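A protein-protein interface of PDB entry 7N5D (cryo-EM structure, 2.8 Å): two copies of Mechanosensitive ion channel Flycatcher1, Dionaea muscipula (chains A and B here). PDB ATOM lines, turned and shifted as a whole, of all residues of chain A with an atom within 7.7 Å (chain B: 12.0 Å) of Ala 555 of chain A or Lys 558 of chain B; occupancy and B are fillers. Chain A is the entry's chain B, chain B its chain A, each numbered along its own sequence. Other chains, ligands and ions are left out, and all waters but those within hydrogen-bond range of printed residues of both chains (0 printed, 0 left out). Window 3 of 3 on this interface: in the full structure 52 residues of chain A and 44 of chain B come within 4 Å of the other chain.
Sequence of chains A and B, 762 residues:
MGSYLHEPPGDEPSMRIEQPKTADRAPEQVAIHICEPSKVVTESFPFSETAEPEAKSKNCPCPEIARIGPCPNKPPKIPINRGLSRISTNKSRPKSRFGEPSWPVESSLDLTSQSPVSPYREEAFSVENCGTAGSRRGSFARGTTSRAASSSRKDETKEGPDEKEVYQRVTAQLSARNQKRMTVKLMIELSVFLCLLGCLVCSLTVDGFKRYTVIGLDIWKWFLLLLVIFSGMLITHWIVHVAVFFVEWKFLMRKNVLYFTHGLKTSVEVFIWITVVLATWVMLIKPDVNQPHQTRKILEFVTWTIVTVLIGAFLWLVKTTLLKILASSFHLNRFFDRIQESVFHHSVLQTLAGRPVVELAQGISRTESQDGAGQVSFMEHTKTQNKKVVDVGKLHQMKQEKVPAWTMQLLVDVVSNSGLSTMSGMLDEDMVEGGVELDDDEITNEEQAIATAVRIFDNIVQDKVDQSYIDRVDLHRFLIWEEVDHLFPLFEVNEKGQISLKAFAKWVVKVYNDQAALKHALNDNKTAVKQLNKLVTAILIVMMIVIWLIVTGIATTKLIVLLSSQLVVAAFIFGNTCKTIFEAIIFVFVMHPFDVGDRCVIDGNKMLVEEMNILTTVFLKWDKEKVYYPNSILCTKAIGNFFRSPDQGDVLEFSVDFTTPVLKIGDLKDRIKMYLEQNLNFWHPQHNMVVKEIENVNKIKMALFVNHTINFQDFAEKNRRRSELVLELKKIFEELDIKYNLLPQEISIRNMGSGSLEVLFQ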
ATOM      1  N   VAL A 546     -14.780 -23.221 -23.298  1.00  0.00           N
ATOM      2  CA  VAL A 546     -14.477 -21.969 -23.918  1.00  0.00           C
ATOM      3  C   VAL A 546     -13.569 -21.160 -23.027  1.00  0.00           C
ATOM      4  O   VAL A 546     -12.626 -20.561 -23.521  1.00  0.00           O
ATOM      5  CB  VAL A 546     -15.725 -21.200 -24.261  1.00  0.00           C
ATOM      6  CG1 VAL A 546     -15.359 -19.792 -24.757  1.00  0.00           C
ATOM      7  CG2 VAL A 546     -16.458 -21.962 -25.310  1.00  0.00           C
ATOM      8  N   TRP A 548     -11.327 -22.193 -20.952  1.00  0.00           N
ATOM      9  CA  TRP A 548      -9.987 -22.734 -21.051  1.00  0.00           C
ATOM     10  C   TRP A 548      -9.304 -22.270 -22.304  1.00  0.00           C
ATOM     11  O   TRP A 548      -8.181 -21.770 -22.272  1.00  0.00           O
ATOM     12  CB  TRP A 548     -10.029 -24.233 -21.081  1.00  0.00           C
ATOM     13  CG  TRP A 548      -8.756 -24.802 -21.171  1.00  0.00           C
ATOM     14  CD1 TRP A 548      -7.874 -24.943 -20.186  1.00  0.00           C
ATOM     15  CD2 TRP A 548      -8.186 -25.397 -22.300  1.00  0.00           C
ATOM     16  NE1 TRP A 548      -6.776 -25.563 -20.642  1.00  0.00           N
ATOM     17  CE2 TRP A 548      -6.953 -25.857 -21.926  1.00  0.00           C
ATOM     18  CE3 TRP A 548      -8.615 -25.589 -23.586  1.00  0.00           C
ATOM     19  CZ2 TRP A 548      -6.137 -26.491 -22.784  1.00  0.00           C
ATOM     20  CZ3 TRP A 548      -7.789 -26.238 -24.461  1.00  0.00           C
ATOM     21  CH2 TRP A 548      -6.577 -26.676 -24.068  1.00  0.00           C
ATOM     22  N   LEU A 549     -10.002 -22.331 -23.417  1.00  0.00           N
ATOM     23  CA  LEU A 549      -9.410 -21.930 -24.665  1.00  0.00           C
ATOM     24  C   LEU A 549      -8.983 -20.480 -24.677  1.00  0.00           C
ATOM     25  O   LEU A 549      -8.000 -20.102 -25.328  1.00  0.00           O
ATOM     26  CB  LEU A 549     -10.408 -22.137 -25.783  1.00  0.00           C
ATOM     27  CG  LEU A 549     -10.729 -23.547 -26.165  1.00  0.00           C
ATOM     28  CD1 LEU A 549     -11.904 -23.535 -27.118  1.00  0.00           C
ATOM     29  CD2 LEU A 549      -9.551 -24.175 -26.838  1.00  0.00           C
ATOM     30  N   ILE A 550      -9.713 -19.646 -23.987  1.00  0.00           N
ATOM     31  CA  ILE A 550      -9.375 -18.254 -23.967  1.00  0.00           C
ATOM     32  C   ILE A 550      -8.329 -17.885 -22.917  1.00  0.00           C
ATOM     33  O   ILE A 550      -7.358 -17.205 -23.235  1.00  0.00           O
ATOM     34  CB  ILE A 550     -10.648 -17.466 -23.731  1.00  0.00           C
ATOM     35  CG1 ILE A 550     -11.655 -17.803 -24.825  1.00  0.00           C
ATOM     36  CG2 ILE A 550     -10.383 -15.976 -23.650  1.00  0.00           C
ATOM     37  CD1 ILE A 550     -11.261 -17.538 -26.219  1.00  0.00           C
ATOM     38  N   VAL A 551      -8.482 -18.329 -21.685  1.00  0.00           N
ATOM     39  CA  VAL A 551      -7.574 -17.921 -20.622  1.00  0.00           C
ATOM     40  C   VAL A 551      -6.168 -18.454 -20.788  1.00  0.00           C
ATOM     41  O   VAL A 551      -5.219 -17.794 -20.380  1.00  0.00           O
ATOM     42  CB  VAL A 551      -8.116 -18.288 -19.237  1.00  0.00           C
ATOM     43  CG1 VAL A 551      -8.009 -19.755 -18.966  1.00  0.00           C
ATOM     44  CG2 VAL A 551      -7.354 -17.522 -18.178  1.00  0.00           C
ATOM     45  N   THR A 552      -5.992 -19.622 -21.395  1.00  0.00           N
ATOM     46  CA  THR A 552      -4.635 -20.110 -21.564  1.00  0.00           C
ATOM     47  C   THR A 552      -3.990 -19.472 -22.782  1.00  0.00           C
ATOM     48  O   THR A 552      -2.807 -19.687 -23.043  1.00  0.00           O
ATOM     49  CB  THR A 552      -4.548 -21.622 -21.783  1.00  0.00           C
ATOM     50  OG1 THR A 552      -5.175 -21.944 -23.015  1.00  0.00           O
ATOM     51  CG2 THR A 552      -5.227 -22.376 -20.668  1.00  0.00           C
ATOM     52  N   GLY A 553      -4.775 -18.774 -23.596  1.00  0.00           N
ATOM     53  CA  GLY A 553      -4.276 -18.147 -24.792  1.00  0.00           C
ATOM     54  C   GLY A 553      -4.136 -19.104 -25.951  1.00  0.00           C
ATOM     55  O   GLY A 553      -3.623 -18.728 -26.999  1.00  0.00           O
ATOM     56  N   ILE A 554      -4.580 -20.336 -25.786  1.00  0.00           N
ATOM     57  CA  ILE A 554      -4.420 -21.301 -26.851  1.00  0.00           C
ATOM     58  C   ILE A 554      -5.227 -20.963 -28.086  1.00  0.00           C
ATOM     59  O   ILE A 554      -4.799 -21.253 -29.200  1.00  0.00           O
ATOM     60  CB  ILE A 554      -4.713 -22.716 -26.333  1.00  0.00           C
ATOM     61  CG1 ILE A 554      -4.234 -23.761 -27.346  1.00  0.00           C
ATOM     62  CG2 ILE A 554      -6.149 -22.879 -25.981  1.00  0.00           C
ATOM     63  CD1 ILE A 554      -4.197 -25.194 -26.804  1.00  0.00           C
ATOM     64  N   ALA A 555      -6.398 -20.388 -27.915  1.00  0.00           N
ATOM     65  CA  ALA A 555      -7.173 -20.005 -29.067  1.00  0.00           C
ATOM     66  C   ALA A 555      -6.669 -18.699 -29.640  1.00  0.00           C
ATOM     67  O   ALA A 555      -6.279 -17.784 -28.912  1.00  0.00           O
ATOM     68  CB  ALA A 555      -8.632 -19.890 -28.705  1.00  0.00           C
ATOM     69  N   THR A 556      -6.780 -18.572 -30.943  1.00  0.00           N
ATOM     70  CA  THR A 556      -6.445 -17.337 -31.603  1.00  0.00           C
ATOM     71  C   THR A 556      -7.692 -16.603 -31.942  1.00  0.00           C
ATOM     72  O   THR A 556      -8.779 -17.174 -31.876  1.00  0.00           O
ATOM     73  CB  THR A 556      -5.648 -17.583 -32.872  1.00  0.00           C
ATOM     74  OG1 THR A 556      -5.231 -16.322 -33.411  1.00  0.00           O
ATOM     75  CG2 THR A 556      -6.503 -18.335 -33.901  1.00  0.00           C
ATOM     76  N   THR A 557      -7.551 -15.380 -32.391  1.00  0.00           N
ATOM     77  CA  THR A 557      -8.712 -14.582 -32.644  1.00  0.00           C
ATOM     78  C   THR A 557      -9.467 -14.816 -33.905  1.00  0.00           C
ATOM     79  O   THR A 557     -10.653 -14.510 -33.971  1.00  0.00           O
ATOM     80  CB  THR A 557      -8.362 -13.111 -32.563  1.00  0.00           C
ATOM     81  OG1 THR A 557      -7.331 -12.826 -33.503  1.00  0.00           O
ATOM     82  CG2 THR A 557      -7.905 -12.794 -31.182  1.00  0.00           C
ATOM     83  N   LYS A 558      -8.863 -15.405 -34.911  1.00  0.00           N
ATOM     84  CA  LYS A 558      -9.673 -15.625 -36.085  1.00  0.00           C
ATOM     85  C   LYS A 558     -10.669 -16.743 -35.838  1.00  0.00           C
ATOM     86  O   LYS A 558     -11.783 -16.741 -36.371  1.00  0.00           O
ATOM     87  CB  LYS A 558      -8.845 -16.004 -37.292  1.00  0.00           C
ATOM     88  CG  LYS A 558      -9.659 -16.195 -38.582  1.00  0.00           C
ATOM     89  CD  LYS A 558     -10.252 -14.880 -39.091  1.00  0.00           C
ATOM     90  CE  LYS A 558     -11.059 -15.080 -40.374  1.00  0.00           C
ATOM     91  NZ  LYS A 558     -10.186 -15.524 -41.504  1.00  0.00           N
ATOM     92  N   LEU A 559     -10.261 -17.706 -35.020  1.00  0.00           N
ATOM     93  CA  LEU A 559     -11.107 -18.837 -34.754  1.00  0.00           C
ATOM     94  C   LEU A 559     -12.137 -18.416 -33.750  1.00  0.00           C
ATOM     95  O   LEU A 559     -13.264 -18.887 -33.823  1.00  0.00           O
ATOM     96  CB  LEU A 559     -10.362 -20.059 -34.269  1.00  0.00           C
ATOM     97  CG  LEU A 559      -9.376 -20.704 -35.286  1.00  0.00           C
ATOM     98  CD1 LEU A 559      -8.663 -21.854 -34.597  1.00  0.00           C
ATOM     99  CD2 LEU A 559     -10.110 -21.189 -36.547  1.00  0.00           C
ATOM    100  N   ILE A 560     -11.793 -17.517 -32.842  1.00  0.00           N
ATOM    101  CA  ILE A 560     -12.773 -17.045 -31.887  1.00  0.00           C
ATOM    102  C   ILE A 560     -13.842 -16.316 -32.637  1.00  0.00           C
ATOM    103  O   ILE A 560     -15.024 -16.485 -32.346  1.00  0.00           O
ATOM    104  CB  ILE A 560     -12.146 -16.172 -30.830  1.00  0.00           C
ATOM    105  CG1 ILE A 560     -11.264 -17.061 -30.009  1.00  0.00           C
ATOM    106  CG2 ILE A 560     -13.239 -15.481 -29.971  1.00  0.00           C
ATOM    107  CD1 ILE A 560     -10.299 -16.336 -29.159  1.00  0.00           C
ATOM    108  N   VAL A 561     -13.463 -15.497 -33.595  1.00  0.00           N
ATOM    109  CA  VAL A 561     -14.477 -14.824 -34.346  1.00  0.00           C
ATOM    110  C   VAL A 561     -15.333 -15.788 -35.139  1.00  0.00           C
ATOM    111  O   VAL A 561     -16.553 -15.629 -35.147  1.00  0.00           O
ATOM    112  CB  VAL A 561     -13.879 -13.776 -35.244  1.00  0.00           C
ATOM    113  CG1 VAL A 561     -14.944 -13.213 -36.182  1.00  0.00           C
ATOM    114  CG2 VAL A 561     -13.323 -12.680 -34.363  1.00  0.00           C
ATOM    115  N   LEU A 563     -16.037 -18.849 -34.421  1.00  0.00           N
ATOM    116  CA  LEU A 563     -16.821 -19.568 -33.440  1.00  0.00           C
ATOM    117  C   LEU A 563     -18.024 -18.768 -33.010  1.00  0.00           C
ATOM    118  O   LEU A 563     -19.143 -19.293 -32.974  1.00  0.00           O
ATOM    119  CB  LEU A 563     -15.958 -19.826 -32.210  1.00  0.00           C
ATOM    120  CG  LEU A 563     -16.600 -20.496 -31.014  1.00  0.00           C
ATOM    121  CD1 LEU A 563     -17.077 -21.878 -31.387  1.00  0.00           C
ATOM    122  CD2 LEU A 563     -15.572 -20.528 -29.869  1.00  0.00           C
ATOM    123  N   SER A 564     -17.824 -17.489 -32.702  1.00  0.00           N
ATOM    124  CA  SER A 564     -18.935 -16.663 -32.300  1.00  0.00           C
ATOM    125  C   SER A 564     -19.896 -16.433 -33.436  1.00  0.00           C
ATOM    126  O   SER A 564     -21.110 -16.404 -33.223  1.00  0.00           O
ATOM    127  CB  SER A 564     -18.467 -15.346 -31.757  1.00  0.00           C
ATOM    128  OG  SER A 564     -17.830 -15.517 -30.529  1.00  0.00           O
ATOM    129  N   VAL B 546     -20.197  -5.955 -16.628  1.00  0.00           N
ATOM    130  CA  VAL B 546     -19.728  -5.853 -17.982  1.00  0.00           C
ATOM    131  C   VAL B 546     -19.221  -4.475 -18.280  1.00  0.00           C
ATOM    132  O   VAL B 546     -18.179  -4.339 -18.910  1.00  0.00           O
ATOM    133  CB  VAL B 546     -20.797  -6.229 -18.977  1.00  0.00           C
ATOM    134  CG1 VAL B 546     -20.305  -5.925 -20.412  1.00  0.00           C
ATOM    135  CG2 VAL B 546     -21.105  -7.700 -18.806  1.00  0.00           C
ATOM    136  N   LEU B 549     -15.730  -4.030 -16.971  1.00  0.00           N
ATOM    137  CA  LEU B 549     -14.711  -4.728 -17.716  1.00  0.00           C
ATOM    138  C   LEU B 549     -14.371  -4.075 -19.018  1.00  0.00           C
ATOM    139  O   LEU B 549     -13.229  -4.147 -19.475  1.00  0.00           O
ATOM    140  CB  LEU B 549     -15.189  -6.129 -18.051  1.00  0.00           C
ATOM    141  CG  LEU B 549     -15.319  -7.101 -16.926  1.00  0.00           C
ATOM    142  CD1 LEU B 549     -16.038  -8.337 -17.438  1.00  0.00           C
ATOM    143  CD2 LEU B 549     -13.932  -7.472 -16.409  1.00  0.00           C
ATOM    144  N   ILE B 550     -15.333  -3.471 -19.667  1.00  0.00           N
ATOM    145  CA  ILE B 550     -14.985  -2.922 -20.942  1.00  0.00           C
ATOM    146  C   ILE B 550     -14.453  -1.492 -20.860  1.00  0.00           C
ATOM    147  O   ILE B 550     -13.485  -1.166 -21.542  1.00  0.00           O
ATOM    148  CB  ILE B 550     -16.159  -3.100 -21.911  1.00  0.00           C
ATOM    149  CG1 ILE B 550     -17.370  -2.258 -21.511  1.00  0.00           C
ATOM    150  CG2 ILE B 550     -16.533  -4.604 -21.867  1.00  0.00           C
ATOM    151  CD1 ILE B 550     -18.509  -2.266 -22.483  1.00  0.00           C
ATOM    152  N   GLY B 553     -10.769  -1.242 -19.924  1.00  0.00           N
ATOM    153  CA  GLY B 553      -9.792  -1.834 -20.809  1.00  0.00           C
ATOM    154  C   GLY B 553      -9.383  -3.234 -20.402  1.00  0.00           C
ATOM    155  O   GLY B 553      -8.518  -3.830 -21.035  1.00  0.00           O
ATOM    156  N   ILE B 554      -9.989  -3.772 -19.361  1.00  0.00           N
ATOM    157  CA  ILE B 554      -9.612  -5.104 -18.958  1.00  0.00           C
ATOM    158  C   ILE B 554      -9.996  -6.110 -20.000  1.00  0.00           C
ATOM    159  O   ILE B 554      -9.216  -7.002 -20.332  1.00  0.00           O
ATOM    160  CB  ILE B 554     -10.263  -5.485 -17.645  1.00  0.00           C
ATOM    161  CG1 ILE B 554      -9.674  -4.638 -16.565  1.00  0.00           C
ATOM    162  CG2 ILE B 554     -10.077  -6.983 -17.370  1.00  0.00           C
ATOM    163  CD1 ILE B 554     -10.431  -4.682 -15.283  1.00  0.00           C
ATOM    164  N   ALA B 555     -11.220  -6.030 -20.487  1.00  0.00           N
ATOM    165  CA  ALA B 555     -11.613  -6.973 -21.498  1.00  0.00           C
ATOM    166  C   ALA B 555     -10.861  -6.666 -22.760  1.00  0.00           C
ATOM    167  O   ALA B 555     -10.807  -5.517 -23.193  1.00  0.00           O
ATOM    168  CB  ALA B 555     -13.102  -6.920 -21.746  1.00  0.00           C
ATOM    169  N   THR B 556     -10.378  -7.698 -23.405  1.00  0.00           N
ATOM    170  CA  THR B 556      -9.672  -7.574 -24.661  1.00  0.00           C
ATOM    171  C   THR B 556     -10.546  -7.891 -25.833  1.00  0.00           C
ATOM    172  O   THR B 556     -11.692  -8.298 -25.668  1.00  0.00           O
ATOM    173  CB  THR B 556      -8.439  -8.453 -24.683  1.00  0.00           C
ATOM    174  OG1 THR B 556      -7.683  -8.163 -25.868  1.00  0.00           O
ATOM    175  CG2 THR B 556      -8.832  -9.898 -24.646  1.00  0.00           C
ATOM    176  N   THR B 557     -10.013  -7.791 -27.034  1.00  0.00           N
ATOM    177  CA  THR B 557     -10.847  -7.995 -28.205  1.00  0.00           C
ATOM    178  C   THR B 557     -11.542  -9.325 -28.210  1.00  0.00           C
ATOM    179  O   THR B 557     -12.734  -9.386 -28.493  1.00  0.00           O
ATOM    180  CB  THR B 557     -10.036  -7.861 -29.488  1.00  0.00           C
ATOM    181  OG1 THR B 557      -9.493  -6.538 -29.565  1.00  0.00           O
ATOM    182  CG2 THR B 557     -10.942  -8.106 -30.692  1.00  0.00           C
ATOM    183  N   LYS B 558     -10.842 -10.400 -27.899  1.00  0.00           N
ATOM    184  CA  LYS B 558     -11.514 -11.684 -27.908  1.00  0.00           C
ATOM    185  C   LYS B 558     -12.588 -11.801 -26.839  1.00  0.00           C
ATOM    186  O   LYS B 558     -13.601 -12.469 -27.053  1.00  0.00           O
ATOM    187  CB  LYS B 558     -10.513 -12.816 -27.805  1.00  0.00           C
ATOM    188  CG  LYS B 558      -9.641 -12.816 -26.587  1.00  0.00           C
ATOM    189  CD  LYS B 558      -8.760 -14.046 -26.482  1.00  0.00           C
ATOM    190  CE  LYS B 558      -7.666 -14.117 -27.530  1.00  0.00           C
ATOM    191  NZ  LYS B 558      -6.643 -15.139 -27.158  1.00  0.00           N
ATOM    192  N   LEU B 559     -12.424 -11.129 -25.716  1.00  0.00           N
ATOM    193  CA  LEU B 559     -13.433 -11.217 -24.695  1.00  0.00           C
ATOM    194  C   LEU B 559     -14.635 -10.430 -25.093  1.00  0.00           C
ATOM    195  O   LEU B 559     -15.752 -10.849 -24.818  1.00  0.00           O
ATOM    196  CB  LEU B 559     -12.897 -10.746 -23.364  1.00  0.00           C
ATOM    197  CG  LEU B 559     -11.809 -11.655 -22.729  1.00  0.00           C
ATOM    198  CD1 LEU B 559     -11.234 -10.973 -21.502  1.00  0.00           C
ATOM    199  CD2 LEU B 559     -12.408 -13.001 -22.327  1.00  0.00           C
ATOM    200  N   ILE B 560     -14.437  -9.335 -25.792  1.00  0.00           N
ATOM    201  CA  ILE B 560     -15.559  -8.552 -26.235  1.00  0.00           C
ATOM    202  C   ILE B 560     -16.357  -9.351 -27.221  1.00  0.00           C
ATOM    203  O   ILE B 560     -17.584  -9.338 -27.169  1.00  0.00           O
ATOM    204  CB  ILE B 560     -15.145  -7.252 -26.905  1.00  0.00           C
ATOM    205  CG1 ILE B 560     -14.407  -6.326 -25.919  1.00  0.00           C
ATOM    206  CG2 ILE B 560     -16.363  -6.572 -27.526  1.00  0.00           C
ATOM    207  CD1 ILE B 560     -15.139  -5.912 -24.699  1.00  0.00           C
ATOM    208  N   VAL B 561     -15.686 -10.050 -28.119  1.00  0.00           N
ATOM    209  CA  VAL B 561     -16.385 -10.847 -29.101  1.00  0.00           C
ATOM    210  C   VAL B 561     -17.214 -11.919 -28.436  1.00  0.00           C
ATOM    211  O   VAL B 561     -18.369 -12.125 -28.818  1.00  0.00           O
ATOM    212  CB  VAL B 561     -15.380 -11.489 -30.071  1.00  0.00           C
ATOM    213  CG1 VAL B 561     -16.049 -12.530 -30.980  1.00  0.00           C
ATOM    214  CG2 VAL B 561     -14.770 -10.406 -30.926  1.00  0.00           C
ATOM    215  N   LEU B 562     -16.662 -12.606 -27.453  1.00  0.00           N
ATOM    216  CA  LEU B 562     -17.439 -13.622 -26.791  1.00  0.00           C
ATOM    217  C   LEU B 562     -18.579 -13.048 -25.975  1.00  0.00           C
ATOM    218  O   LEU B 562     -19.670 -13.609 -25.997  1.00  0.00           O
ATOM    219  CB  LEU B 562     -16.524 -14.448 -25.935  1.00  0.00           C
ATOM    220  CG  LEU B 562     -15.535 -15.318 -26.731  1.00  0.00           C
ATOM    221  CD1 LEU B 562     -14.513 -15.852 -25.813  1.00  0.00           C
ATOM    222  CD2 LEU B 562     -16.259 -16.503 -27.418  1.00  0.00           C
ATOM    223  N   LEU B 563     -18.380 -11.923 -25.296  1.00  0.00           N
ATOM    224  CA  LEU B 563     -19.467 -11.358 -24.526  1.00  0.00           C
ATOM    225  C   LEU B 563     -20.564 -10.910 -25.433  1.00  0.00           C
ATOM    226  O   LEU B 563     -21.738 -11.063 -25.099  1.00  0.00           O
ATOM    227  CB  LEU B 563     -19.015 -10.139 -23.735  1.00  0.00           C
ATOM    228  CG  LEU B 563     -18.090 -10.356 -22.567  1.00  0.00           C
ATOM    229  CD1 LEU B 563     -17.572  -8.984 -22.091  1.00  0.00           C
ATOM    230  CD2 LEU B 563     -18.832 -11.050 -21.442  1.00  0.00           C
ATOM    231  N   SER B 564     -20.198 -10.355 -26.581  1.00  0.00           N
ATOM    232  CA  SER B 564     -21.169  -9.871 -27.520  1.00  0.00           C
ATOM    233  C   SER B 564     -22.024 -11.004 -28.001  1.00  0.00           C
ATOM    234  O   SER B 564     -23.254 -10.897 -28.025  1.00  0.00           O
ATOM    235  CB  SER B 564     -20.477  -9.217 -28.677  1.00  0.00           C
ATOM    236  OG  SER B 564     -21.398  -8.746 -29.610  1.00  0.00           O
ATOM    237  N   SER B 565     -21.400 -12.121 -28.327  1.00  0.00           N
ATOM    238  CA  SER B 565     -22.148 -13.267 -28.771  1.00  0.00           C
ATOM    239  C   SER B 565     -23.068 -13.757 -27.671  1.00  0.00           C
ATOM    240  O   SER B 565     -24.249 -14.008 -27.896  1.00  0.00           O
ATOM    241  CB  SER B 565     -21.202 -14.359 -29.164  1.00  0.00           C
ATOM    242  OG  SER B 565     -21.887 -15.477 -29.629  1.00  0.00           O
ATOM    243  N   GLN B 566     -22.579 -13.822 -26.438  1.00  0.00           N
ATOM    244  CA  GLN B 566     -23.410 -14.332 -25.368  1.00  0.00           C
ATOM    245  C   GLN B 566     -24.643 -13.489 -25.179  1.00  0.00           C
ATOM    246  O   GLN B 566     -25.729 -14.028 -24.961  1.00  0.00           O
ATOM    247  CB  GLN B 566     -22.621 -14.366 -24.084  1.00  0.00           C
ATOM    248  CG  GLN B 566     -21.543 -15.412 -24.061  1.00  0.00           C
ATOM    249  CD  GLN B 566     -20.621 -15.244 -22.872  1.00  0.00           C
ATOM    250  OE1 GLN B 566     -20.654 -14.201 -22.212  1.00  0.00           O
ATOM    251  NE2 GLN B 566     -19.803 -16.250 -22.591  1.00  0.00           N
ATOM    252  N   LEU B 567     -24.513 -12.183 -25.303  1.00  0.00           N
ATOM    253  CA  LEU B 567     -25.665 -11.342 -25.167  1.00  0.00           C
ATOM    254  C   LEU B 567     -26.647 -11.577 -26.284  1.00  0.00           C
ATOM    255  O   LEU B 567     -27.849 -11.648 -26.037  1.00  0.00           O
ATOM    256  CB  LEU B 567     -25.257  -9.887 -25.142  1.00  0.00           C
ATOM    257  CG  LEU B 567     -26.385  -8.851 -25.019  1.00  0.00           C
ATOM    258  CD1 LEU B 567     -27.195  -9.067 -23.756  1.00  0.00           C
ATOM    259  CD2 LEU B 567     -25.755  -7.467 -25.000  1.00  0.00           C
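No residue of chain B comes within 4 Å of Leu 549 of chain A. No residue of chain B comes within 4 Å of Gly 553 of chain A. Ala 555 of chain A touches just one residue of chain B: Lys 558 (3.2 Å). No residue of chain B comes within 4 Å of Thr 556 of chain A. Thr 557 of chain A touches just one residue of chain B: Lys 558 (3.9 Å). Of chain B, only Lys 558 (3.8 Å) and Leu 562 (3.97 Å) come within 4 Å of Ile 560 of chain A. Of the printed residues of chain B, Ser 564 of chain A touches Val 561, Leu 562 and Ser 565. Gly 553 of chain B touches none of the printed residues of chain A. Thr 556 of chain B touches none of the printed residues of chain A. Of chain A, only Ile 550 (3.8 Å), Ala 555 (3.2 Å), Thr 557 (3.9 Å) and Ile 560 (3.8 Å) come within 4 Å of Lys 558 of chain B. Of the printed residues of chain A, Leu 559 of chain B touches Ile 550 (3.8 Å). Printed residues of chain A within 4 Å of Leu 562 of chain B: Ile 550 (3.6 Å), Ile 560 (3.97 Å) and Ser 564 (3.6 Å). Of the printed residues of chain A, Ser 565 of chain B touches Ser 564. The nearest printed residue of chain B that does not touch Ser 564 of chain A is Lys 558 of chain B (6.3 Å).
Hydrophobic or aromatic side chains of chain B within 4 Å of the printed part of chain A: Leu 559, Val 561 and Leu 562. Of the 17 printed residues of chain A, 5 touch a printed residue of chain B. Hydrophobic or aromatic side chains of chain A that line the printed part of chain B: Ile 550 and Ile 560. Along chain A the printed residues that touch a printed residue of chain B span positions 550 to 564. Among the printed residues, 10 pairs touch across the chains. Among the printed residues, no Asp or Glu carboxylate lies within 4 Å of a Lys or Arg side-chain nitrogen of the other chain.
Ile 550 of chain A touches Lys 558 of chain B. Ile 550 of chain A touches Leu 559 of chain B (CG2 to CD2, 3.8 Å). Ile 550 of chain A touches Leu 562 of chain B (CG1 to CD1, 3.6 Å). Thr 557 of chain A touches Lys 558 of chain B (CG2 to CE, 3.9 Å). Lys 558 of chain B touches Ile 560 of chain A (CB to CD1, 3.8 Å). CG2 of Ile 560 of chain A touches CG of Leu 562 of chain B, 3.97 Å away. Ser 564 of chain A touches Val 561 of chain B. Ser 564 of chain A touches Leu 562 of chain B (OG to CD2, 3.6 Å). Ser 565 of chain B touches Ser 564 of chain A.
The backbone carbonyl oxygen (O) of Ile 560 of chain A lies within hydrogen-bond range of the side-chain hydroxyl (OG) of Ser 564 of chain A (3.5 Å). The backbone NH (N) of Ala 555 of chain A is in hydrogen-bond range of the backbone carbonyl oxygen (O) of Leu 549 of chain A.
O of Ala 555 of chain A lies within hydrogen-bond range of NZ of Lys 558 of chain B (3.2 Å).
Ile 550 of chain A touches Lys 558 of chain B, but with the chains exchanged Lys 558 of chain A does not touch Ile 550 of chain B (18.6 Å). Ala 555 of chain A touches Lys 558 of chain B, but with the chains exchanged Lys 558 of chain A does not touch Ala 555 of chain B (15.1 Å). Thr 557 of chain A touches Lys 558 of chain B, but with the chains exchanged Lys 558 of chain A does not touch Thr 557 of chain B (8.7 Å). Ile 560 of chain A touches Lys 558 of chain B, but with the chains exchanged Lys 558 of chain A does not touch Ile 560 of chain B (12.3 Å).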
